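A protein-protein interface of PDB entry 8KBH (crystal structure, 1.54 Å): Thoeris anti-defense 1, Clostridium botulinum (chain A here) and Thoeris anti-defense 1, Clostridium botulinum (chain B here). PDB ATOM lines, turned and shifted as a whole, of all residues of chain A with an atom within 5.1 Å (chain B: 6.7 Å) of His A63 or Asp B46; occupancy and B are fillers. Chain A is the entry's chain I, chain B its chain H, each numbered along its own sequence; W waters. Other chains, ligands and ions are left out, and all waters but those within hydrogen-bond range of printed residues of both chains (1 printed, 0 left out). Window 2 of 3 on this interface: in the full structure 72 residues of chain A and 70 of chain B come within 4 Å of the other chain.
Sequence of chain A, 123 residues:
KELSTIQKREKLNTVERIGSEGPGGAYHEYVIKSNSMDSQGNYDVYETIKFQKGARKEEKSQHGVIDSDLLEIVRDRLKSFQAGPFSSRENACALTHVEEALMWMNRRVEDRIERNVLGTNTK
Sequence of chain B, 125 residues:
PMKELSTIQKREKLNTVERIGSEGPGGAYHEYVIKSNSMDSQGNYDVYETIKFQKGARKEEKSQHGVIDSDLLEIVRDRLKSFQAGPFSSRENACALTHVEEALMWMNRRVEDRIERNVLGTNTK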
ATOM      1  N   PHE A  51     -12.304  14.399  -9.057  1.00  0.00           N
ATOM      2  CA  PHE A  51     -13.707  14.697  -8.817  1.00  0.00           C
ATOM      3  C   PHE A  51     -14.587  13.580  -9.367  1.00  0.00           C
ATOM      4  O   PHE A  51     -14.231  12.904 -10.336  1.00  0.00           O
ATOM      5  CB  PHE A  51     -14.101  16.028  -9.460  1.00  0.00           C
ATOM      6  CG  PHE A  51     -13.547  17.231  -8.751  1.00  0.00           C
ATOM      7  CD1 PHE A  51     -12.236  17.638  -8.958  1.00  0.00           C
ATOM      8  CD2 PHE A  51     -14.341  17.950  -7.870  1.00  0.00           C
ATOM      9  CE1 PHE A  51     -11.733  18.746  -8.297  1.00  0.00           C
ATOM     10  CE2 PHE A  51     -13.841  19.056  -7.200  1.00  0.00           C
ATOM     11  CZ  PHE A  51     -12.547  19.454  -7.416  1.00  0.00           C
ATOM     12  N   GLN A  52     -15.741  13.390  -8.736  1.00  0.00           N
ATOM     13  CA  GLN A  52     -16.768  12.529  -9.310  1.00  0.00           C
ATOM     14  C   GLN A  52     -16.996  12.884 -10.773  1.00  0.00           C
ATOM     15  O   GLN A  52     -17.320  14.028 -11.101  1.00  0.00           O
ATOM     16  CB  GLN A  52     -18.067  12.676  -8.517  1.00  0.00           C
ATOM     17  CG  GLN A  52     -19.131  11.660  -8.907  1.00  0.00           C
ATOM     18  CD  GLN A  52     -18.723  10.249  -8.541  1.00  0.00           C
ATOM     19  OE1 GLN A  52     -18.118  10.023  -7.498  1.00  0.00           O
ATOM     20  NE2 GLN A  52     -19.044   9.297  -9.406  1.00  0.00           N
ATOM     21  N   LYS A  53     -16.801  11.908 -11.657  1.00  0.00           N
ATOM     22  CA  LYS A  53     -16.951  12.100 -13.097  1.00  0.00           C
ATOM     23  C   LYS A  53     -17.808  10.949 -13.609  1.00  0.00           C
ATOM     24  O   LYS A  53     -17.341   9.809 -13.677  1.00  0.00           O
ATOM     25  CB  LYS A  53     -15.581  12.150 -13.786  1.00  0.00           C
ATOM     26  CG  LYS A  53     -15.565  12.413 -15.296  1.00  0.00           C
ATOM     27  CD  LYS A  53     -14.149  12.160 -15.853  1.00  0.00           C
ATOM     28  CE  LYS A  53     -14.051  12.402 -17.355  1.00  0.00           C
ATOM     29  NZ  LYS A  53     -12.664  12.799 -17.783  1.00  0.00           N
ATOM     30  N   ALA A  55     -22.028   9.403 -13.017  1.00  0.00           N
ATOM     31  CA  ALA A  55     -22.910   9.173 -11.882  1.00  0.00           C
ATOM     32  C   ALA A  55     -22.321   8.159 -10.906  1.00  0.00           C
ATOM     33  O   ALA A  55     -21.676   7.185 -11.303  1.00  0.00           O
ATOM     34  CB  ALA A  55     -24.274   8.695 -12.371  1.00  0.00           C
ATOM     35  N   ARG A  56     -22.562   8.400  -9.616  1.00  0.00           N
ATOM     36  CA  ARG A  56     -22.033   7.539  -8.565  1.00  0.00           C
ATOM     37  C   ARG A  56     -22.669   6.152  -8.582  1.00  0.00           C
ATOM     38  O   ARG A  56     -22.042   5.183  -8.133  1.00  0.00           O
ATOM     39  CB  ARG A  56     -22.239   8.220  -7.207  1.00  0.00           C
ATOM     40  CG  ARG A  56     -21.933   7.376  -5.972  1.00  0.00           C
ATOM     41  CD  ARG A  56     -20.455   7.031  -5.848  1.00  0.00           C
ATOM     42  NE  ARG A  56     -19.589   8.199  -5.700  1.00  0.00           N
ATOM     43  CZ  ARG A  56     -19.378   8.839  -4.552  1.00  0.00           C
ATOM     44  NH1 ARG A  56     -19.992   8.452  -3.438  1.00  0.00           N
ATOM     45  NH2 ARG A  56     -18.564   9.884  -4.521  1.00  0.00           N
ATOM     46  N   LYS A  57     -23.897   6.018  -9.096  1.00  0.00           N
ATOM     47  CA  LYS A  57     -24.500   4.690  -9.142  1.00  0.00           C
ATOM     48  C   LYS A  57     -23.857   3.800 -10.199  1.00  0.00           C
ATOM     49  O   LYS A  57     -23.984   2.574 -10.112  1.00  0.00           O
ATOM     50  CB  LYS A  57     -26.002   4.774  -9.414  1.00  0.00           C
ATOM     51  CG  LYS A  57     -26.353   5.281 -10.801  1.00  0.00           C
ATOM     52  CD  LYS A  57     -27.858   5.297 -11.031  1.00  0.00           C
ATOM     53  CE  LYS A  57     -28.185   5.782 -12.432  1.00  0.00           C
ATOM     54  NZ  LYS A  57     -29.643   5.816 -12.700  1.00  0.00           N
ATOM     55  N   GLU A  58     -23.184   4.381 -11.195  1.00  0.00           N
ATOM     56  CA  GLU A  58     -22.561   3.612 -12.268  1.00  0.00           C
ATOM     57  C   GLU A  58     -21.153   3.183 -11.870  1.00  0.00           C
ATOM     58  O   GLU A  58     -20.334   4.014 -11.468  1.00  0.00           O
ATOM     59  CB  GLU A  58     -22.514   4.425 -13.564  1.00  0.00           C
ATOM     60  CG  GLU A  58     -23.862   4.941 -14.034  1.00  0.00           C
ATOM     61  CD  GLU A  58     -23.864   5.313 -15.509  1.00  0.00           C
ATOM     62  OE1 GLU A  58     -24.592   4.663 -16.286  1.00  0.00           O
ATOM     63  OE2 GLU A  58     -23.140   6.256 -15.893  1.00  0.00           O
ATOM     64  N   GLU A  59     -20.869   1.883 -12.009  1.00  0.00           N
ATOM     65  CA  GLU A  59     -19.582   1.347 -11.578  1.00  0.00           C
ATOM     66  C   GLU A  59     -18.424   1.825 -12.449  1.00  0.00           C
ATOM     67  O   GLU A  59     -17.286   1.856 -11.972  1.00  0.00           O
ATOM     68  CB  GLU A  59     -19.631  -0.189 -11.554  1.00  0.00           C
ATOM     69  CG  GLU A  59     -20.227  -0.824 -12.806  1.00  0.00           C
ATOM     70  CD  GLU A  59     -20.683  -2.264 -12.604  1.00  0.00           C
ATOM     71  OE1 GLU A  59     -20.409  -2.846 -11.530  1.00  0.00           O
ATOM     72  OE2 GLU A  59     -21.316  -2.817 -13.532  1.00  0.00           O
ATOM     73  N   SER A  61     -17.897   4.866 -13.507  1.00  0.00           N
ATOM     74  CA  SER A  61     -17.572   6.274 -13.334  1.00  0.00           C
ATOM     75  C   SER A  61     -16.251   6.438 -12.587  1.00  0.00           C
ATOM     76  O   SER A  61     -15.801   5.543 -11.866  1.00  0.00           O
ATOM     77  CB  SER A  61     -18.688   6.993 -12.574  1.00  0.00           C
ATOM     78  OG  SER A  61     -19.912   6.928 -13.285  1.00  0.00           O
ATOM     79  N   GLN A  62     -15.623   7.599 -12.772  1.00  0.00           N
ATOM     80  CA  GLN A  62     -14.521   8.001 -11.899  1.00  0.00           C
ATOM     81  C   GLN A  62     -15.144   8.577 -10.635  1.00  0.00           C
ATOM     82  O   GLN A  62     -15.647   9.701 -10.633  1.00  0.00           O
ATOM     83  CB  GLN A  62     -13.594   9.006 -12.573  1.00  0.00           C
ATOM     84  CG  GLN A  62     -12.565   9.627 -11.592  1.00  0.00           C
ATOM     85  CD  GLN A  62     -11.691  10.719 -12.206  1.00  0.00           C
ATOM     86  OE1 GLN A  62     -10.945  10.474 -13.162  1.00  0.00           O
ATOM     87  NE2 GLN A  62     -11.768  11.932 -11.648  1.00  0.00           N
ATOM     88  N   HIS A  63     -15.144   7.792  -9.561  1.00  0.00           N
ATOM     89  CA  HIS A  63     -15.673   8.258  -8.291  1.00  0.00           C
ATOM     90  C   HIS A  63     -14.672   9.181  -7.611  1.00  0.00           C
ATOM     91  O   HIS A  63     -13.466   8.919  -7.609  1.00  0.00           O
ATOM     92  CB  HIS A  63     -16.017   7.072  -7.395  1.00  0.00           C
ATOM     93  CG  HIS A  63     -17.001   6.131  -8.012  1.00  0.00           C
ATOM     94  ND1 HIS A  63     -18.220   6.549  -8.503  1.00  0.00           N
ATOM     95  CD2 HIS A  63     -16.933   4.800  -8.257  1.00  0.00           C
ATOM     96  CE1 HIS A  63     -18.870   5.514  -9.004  1.00  0.00           C
ATOM     97  NE2 HIS A  63     -18.112   4.441  -8.865  1.00  0.00           N
ATOM     98  N   GLY A  64     -15.173  10.279  -7.059  1.00  0.00           N
ATOM     99  CA  GLY A  64     -14.274  11.241  -6.453  1.00  0.00           C
ATOM    100  C   GLY A  64     -15.009  12.256  -5.608  1.00  0.00           C
ATOM    101  O   GLY A  64     -16.173  12.072  -5.245  1.00  0.00           O
ATOM    102  N   VAL A  65     -14.297  13.338  -5.291  1.00  0.00           N
ATOM    103  CA  VAL A  65     -14.831  14.385  -4.426  1.00  0.00           C
ATOM    104  C   VAL A  65     -15.806  15.235  -5.224  1.00  0.00           C
ATOM    105  O   VAL A  65     -15.911  15.103  -6.448  1.00  0.00           O
ATOM    106  CB  VAL A  65     -13.714  15.261  -3.826  1.00  0.00           C
ATOM    107  CG1 VAL A  65     -12.639  14.400  -3.131  1.00  0.00           C
ATOM    108  CG2 VAL A  65     -13.113  16.155  -4.889  1.00  0.00           C
ATOM    109  N   ASN B  15     -20.509  12.258  -0.274  1.00  0.00           N
ATOM    110  CA  ASN B  15     -19.407  11.934   0.614  1.00  0.00           C
ATOM    111  C   ASN B  15     -19.606  12.618   1.957  1.00  0.00           C
ATOM    112  O   ASN B  15     -20.354  13.588   2.087  1.00  0.00           O
ATOM    113  CB  ASN B  15     -18.058  12.357   0.018  1.00  0.00           C
ATOM    114  CG  ASN B  15     -17.919  11.995  -1.446  1.00  0.00           C
ATOM    115  OD1 ASN B  15     -18.057  10.834  -1.832  1.00  0.00           O
ATOM    116  ND2 ASN B  15     -17.636  12.998  -2.275  1.00  0.00           N
ATOM    117  N   SER B  36     -16.459   8.289   0.799  1.00  0.00           N
ATOM    118  CA  SER B  36     -17.719   8.127   0.094  1.00  0.00           C
ATOM    119  C   SER B  36     -18.798   7.524   0.982  1.00  0.00           C
ATOM    120  O   SER B  36     -18.532   6.678   1.842  1.00  0.00           O
ATOM    121  CB  SER B  36     -17.519   7.254  -1.143  1.00  0.00           C
ATOM    122  OG  SER B  36     -17.013   5.976  -0.797  1.00  0.00           O
ATOM    123  N   ASN B  37     -20.043   7.952   0.737  1.00  0.00           N
ATOM    124  CA  ASN B  37     -21.202   7.345   1.382  1.00  0.00           C
ATOM    125  C   ASN B  37     -21.676   6.103   0.643  1.00  0.00           C
ATOM    126  O   ASN B  37     -22.850   5.724   0.724  1.00  0.00           O
ATOM    127  CB  ASN B  37     -22.339   8.360   1.508  1.00  0.00           C
ATOM    128  CG  ASN B  37     -21.990   9.501   2.442  1.00  0.00           C
ATOM    129  OD1 ASN B  37     -21.285   9.311   3.434  1.00  0.00           O
ATOM    130  ND2 ASN B  37     -22.471  10.697   2.123  1.00  0.00           N
ATOM    131  N   SER B  38     -20.764   5.481  -0.095  1.00  0.00           N
ATOM    132  CA  SER B  38     -21.039   4.295  -0.884  1.00  0.00           C
ATOM    133  C   SER B  38     -19.836   3.371  -0.801  1.00  0.00           C
ATOM    134  O   SER B  38     -18.709   3.807  -0.541  1.00  0.00           O
ATOM    135  CB  SER B  38     -21.339   4.654  -2.345  1.00  0.00           C
ATOM    136  OG  SER B  38     -20.291   5.437  -2.899  1.00  0.00           O
ATOM    137  N   MET B  39     -20.082   2.084  -1.027  1.00  0.00           N
ATOM    138  CA  MET B  39     -19.027   1.089  -0.973  1.00  0.00           C
ATOM    139  C   MET B  39     -18.958   0.393  -2.322  1.00  0.00           C
ATOM    140  O   MET B  39     -19.960   0.309  -3.042  1.00  0.00           O
ATOM    141  CB  MET B  39     -19.284   0.071   0.135  1.00  0.00           C
ATOM    142  CG  MET B  39     -19.146   0.717   1.487  1.00  0.00           C
ATOM    143  SD  MET B  39     -17.660   1.718   1.640  1.00  0.00           S
ATOM    144  CE  MET B  39     -17.832   2.234   3.344  1.00  0.00           C
ATOM    145  N   ASP B  40     -17.771  -0.092  -2.674  1.00  0.00           N
ATOM    146  CA  ASP B  40     -17.601  -0.717  -3.976  1.00  0.00           C
ATOM    147  C   ASP B  40     -18.129  -2.152  -3.918  1.00  0.00           C
ATOM    148  O   ASP B  40     -18.722  -2.585  -2.923  1.00  0.00           O
ATOM    149  CB  ASP B  40     -16.147  -0.601  -4.438  1.00  0.00           C
ATOM    150  CG  ASP B  40     -15.188  -1.494  -3.662  1.00  0.00           C
ATOM    151  OD1 ASP B  40     -15.599  -2.146  -2.681  1.00  0.00           O
ATOM    152  OD2 ASP B  40     -13.996  -1.536  -4.045  1.00  0.00           O
ATOM    153  N   SER B  41     -17.929  -2.904  -5.001  1.00  0.00           N
ATOM    154  CA  SER B  41     -18.490  -4.246  -5.080  1.00  0.00           C
ATOM    155  C   SER B  41     -17.868  -5.182  -4.051  1.00  0.00           C
ATOM    156  O   SER B  41     -18.514  -6.145  -3.620  1.00  0.00           O
ATOM    157  CB  SER B  41     -18.311  -4.802  -6.494  1.00  0.00           C
ATOM    158  OG  SER B  41     -16.936  -4.953  -6.804  1.00  0.00           O
ATOM    159  N   ASN B  44     -15.360  -1.830  -0.215  1.00  0.00           N
ATOM    160  CA  ASN B  44     -14.405  -0.775   0.089  1.00  0.00           C
ATOM    161  C   ASN B  44     -14.953   0.584  -0.336  1.00  0.00           C
ATOM    162  O   ASN B  44     -15.851   0.685  -1.178  1.00  0.00           O
ATOM    163  CB  ASN B  44     -13.067  -1.038  -0.610  1.00  0.00           C
ATOM    164  CG  ASN B  44     -12.556  -2.445  -0.374  1.00  0.00           C
ATOM    165  OD1 ASN B  44     -12.512  -3.266  -1.294  1.00  0.00           O
ATOM    166  ND2 ASN B  44     -12.195  -2.741   0.866  1.00  0.00           N
ATOM    167  N   TYR B  45     -14.385   1.632   0.259  1.00  0.00           N
ATOM    168  CA  TYR B  45     -14.744   3.009  -0.076  1.00  0.00           C
ATOM    169  C   TYR B  45     -14.513   3.291  -1.558  1.00  0.00           C
ATOM    170  O   TYR B  45     -13.403   3.103  -2.068  1.00  0.00           O
ATOM    171  CB  TYR B  45     -13.914   3.968   0.781  1.00  0.00           C
ATOM    172  CG  TYR B  45     -14.432   4.195   2.189  1.00  0.00           C
ATOM    173  CD1 TYR B  45     -15.620   4.889   2.422  1.00  0.00           C
ATOM    174  CD2 TYR B  45     -13.702   3.763   3.292  1.00  0.00           C
ATOM    175  CE1 TYR B  45     -16.080   5.112   3.714  1.00  0.00           C
ATOM    176  CE2 TYR B  45     -14.160   3.977   4.586  1.00  0.00           C
ATOM    177  CZ  TYR B  45     -15.349   4.647   4.790  1.00  0.00           C
ATOM    178  OH  TYR B  45     -15.797   4.865   6.076  1.00  0.00           O
ATOM    179  N   ASP B  46     -15.564   3.742  -2.255  1.00  0.00           N
ATOM    180  CA  ASP B  46     -15.374   4.275  -3.602  1.00  0.00           C
ATOM    181  C   ASP B  46     -14.461   5.494  -3.588  1.00  0.00           C
ATOM    182  O   ASP B  46     -13.769   5.766  -4.573  1.00  0.00           O
ATOM    183  CB  ASP B  46     -16.716   4.669  -4.229  1.00  0.00           C
ATOM    184  CG  ASP B  46     -17.592   3.475  -4.560  1.00  0.00           C
ATOM    185  OD1 ASP B  46     -17.108   2.529  -5.225  1.00  0.00           O
ATOM    186  OD2 ASP B  46     -18.775   3.493  -4.155  1.00  0.00           O
ATOM    187  N   VAL B  47     -14.481   6.256  -2.499  1.00  0.00           N
ATOM    188  CA  VAL B  47     -13.697   7.478  -2.362  1.00  0.00           C
ATOM    189  C   VAL B  47     -13.123   7.512  -0.953  1.00  0.00           C
ATOM    190  O   VAL B  47     -13.828   7.236   0.022  1.00  0.00           O
ATOM    191  CB  VAL B  47     -14.550   8.737  -2.640  1.00  0.00           C
ATOM    192  CG1 VAL B  47     -13.721  10.002  -2.499  1.00  0.00           C
ATOM    193  CG2 VAL B  47     -15.164   8.680  -4.029  1.00  0.00           C
ATOM    194  N   TYR B  48     -11.832   7.834  -0.856  1.00  0.00           N
ATOM    195  CA  TYR B  48     -11.158   7.969   0.436  1.00  0.00           C
ATOM    196  C   TYR B  48      -9.934   8.856   0.198  1.00  0.00           C
ATOM    197  O   TYR B  48      -8.882   8.356  -0.197  1.00  0.00           O
ATOM    198  CB  TYR B  48     -10.754   6.623   1.013  1.00  0.00           C
ATOM    199  CG  TYR B  48     -10.334   6.749   2.454  1.00  0.00           C
ATOM    200  CD1 TYR B  48     -11.274   6.798   3.473  1.00  0.00           C
ATOM    201  CD2 TYR B  48      -8.997   6.902   2.786  1.00  0.00           C
ATOM    202  CE1 TYR B  48     -10.882   6.945   4.790  1.00  0.00           C
ATOM    203  CE2 TYR B  48      -8.596   7.055   4.103  1.00  0.00           C
ATOM    204  CZ  TYR B  48      -9.545   7.074   5.101  1.00  0.00           C
ATOM    205  OH  TYR B  48      -9.164   7.227   6.416  1.00  0.00           O
ATOM    206  N   GLU B  49     -10.086  10.153   0.443  1.00  0.00           N
ATOM    207  CA  GLU B  49      -9.188  11.140  -0.143  1.00  0.00           C
ATOM    208  C   GLU B  49      -8.687  12.054   0.963  1.00  0.00           C
ATOM    209  O   GLU B  49      -9.489  12.658   1.677  1.00  0.00           O
ATOM    210  CB  GLU B  49      -9.923  11.961  -1.200  1.00  0.00           C
ATOM    211  CG  GLU B  49     -10.475  11.145  -2.363  1.00  0.00           C
ATOM    212  CD  GLU B  49      -9.593   9.984  -2.808  1.00  0.00           C
ATOM    213  OE1 GLU B  49      -8.442  10.215  -3.235  1.00  0.00           O
ATOM    214  OE2 GLU B  49     -10.072   8.824  -2.733  1.00  0.00           O
HETATM  215  O   HOH W   1     -22.753   7.596  -2.351  1.00  0.00           O
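Printed residues of chain A that touch a printed residue of chain B: Arg A56, His A63, Gly A64 and Val A65. Printed residues of chain B that touch a printed residue of chain A: Asn B15, Ser B36, Ser B38, Asp B46, Val B47 and Glu B49. Along chain B the printed residues that touch a printed residue of chain A span positions 15 to 49. Among the printed residues, 10 pairs touch across the chains.
NH2 of Arg A56 lies within hydrogen-bond range of OD1 of Asn B15 (2.9 Å). O of Gly A64 is in hydrogen-bond range of ND2 of Asn B15 (3.4 Å). OG of Ser B38 sits at hydrogen-bond distance from NH1 of Arg A56 (3.1 Å).
The backbone NH of Asn B15 sits close to the side-chain amide nitrogen of Asn B37 (3.5 Å). The side-chain hydroxyl of Ser B38 sits at hydrogen-bond distance from the side-chain carboxylate of Asp B46 (2.8 Å). A ring nitrogen (ND1) of His A63 is in hydrogen-bond range of the side-chain amide nitrogen of Gln A52. The backbone NH of Gly A64 sits at hydrogen-bond distance from the side-chain amide oxygen of Gln A52, at 3.0 Å. The backbone carbonyl oxygen (O) of Val A65 is in hydrogen-bond range of the backbone NH (N) of Gln A52, at 2.9 Å. O of Glu A58 sits close to NE2 of His A63 (3.4 Å).
Water W1 lies within hydrogen-bond range of the guanidinium group (NH1) of Arg A56 and the side-chain hydroxyl (OG) of Ser B38.
Among the printed residues, merely in contact across the chains: Gly A64 with Val B47 (3.4 Å), Arg A56 with Ser B36 (3.6 Å), Arg A56 with Val B47 (3.6 Å), His A63 with Val B47 (3.7 Å), His A63 with Asp B46 (3.8 Å), Val A65 with Asn B15 (3.8 Å) and Val A65 with Glu B49 (3.98 Å).
His A63 touches just these residues of chain B: Asp B46 (3.8 Å) and Val B47 (3.7 Å). Of chain A, only His A63 comes within 4 Å of Asp B46. Printed residues of chain B within 4 Å of Gly A64: Asn B15 (3.4 Å) and Val B47 (3.4 Å). Printed residues of chain B within 4 Å of Val A65: Asn B15 and Glu B49. Of the printed residues of chain A, Glu B49 touches Val A65 (3.98 Å). Printed residues of chain A within 4 Å of Ser B38: Arg A56. Of the printed residues of chain A, Ser B36 touches Arg A56. The nearest residue of chain B that does not touch His A63 is Glu B49 (5.9 Å). The nearest residue of chain A that does not touch Asp B46 is Arg A56 (4.3 Å). The nearest printed residue of chain A that does not touch Ser B38 is His A63 (6.1 Å).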
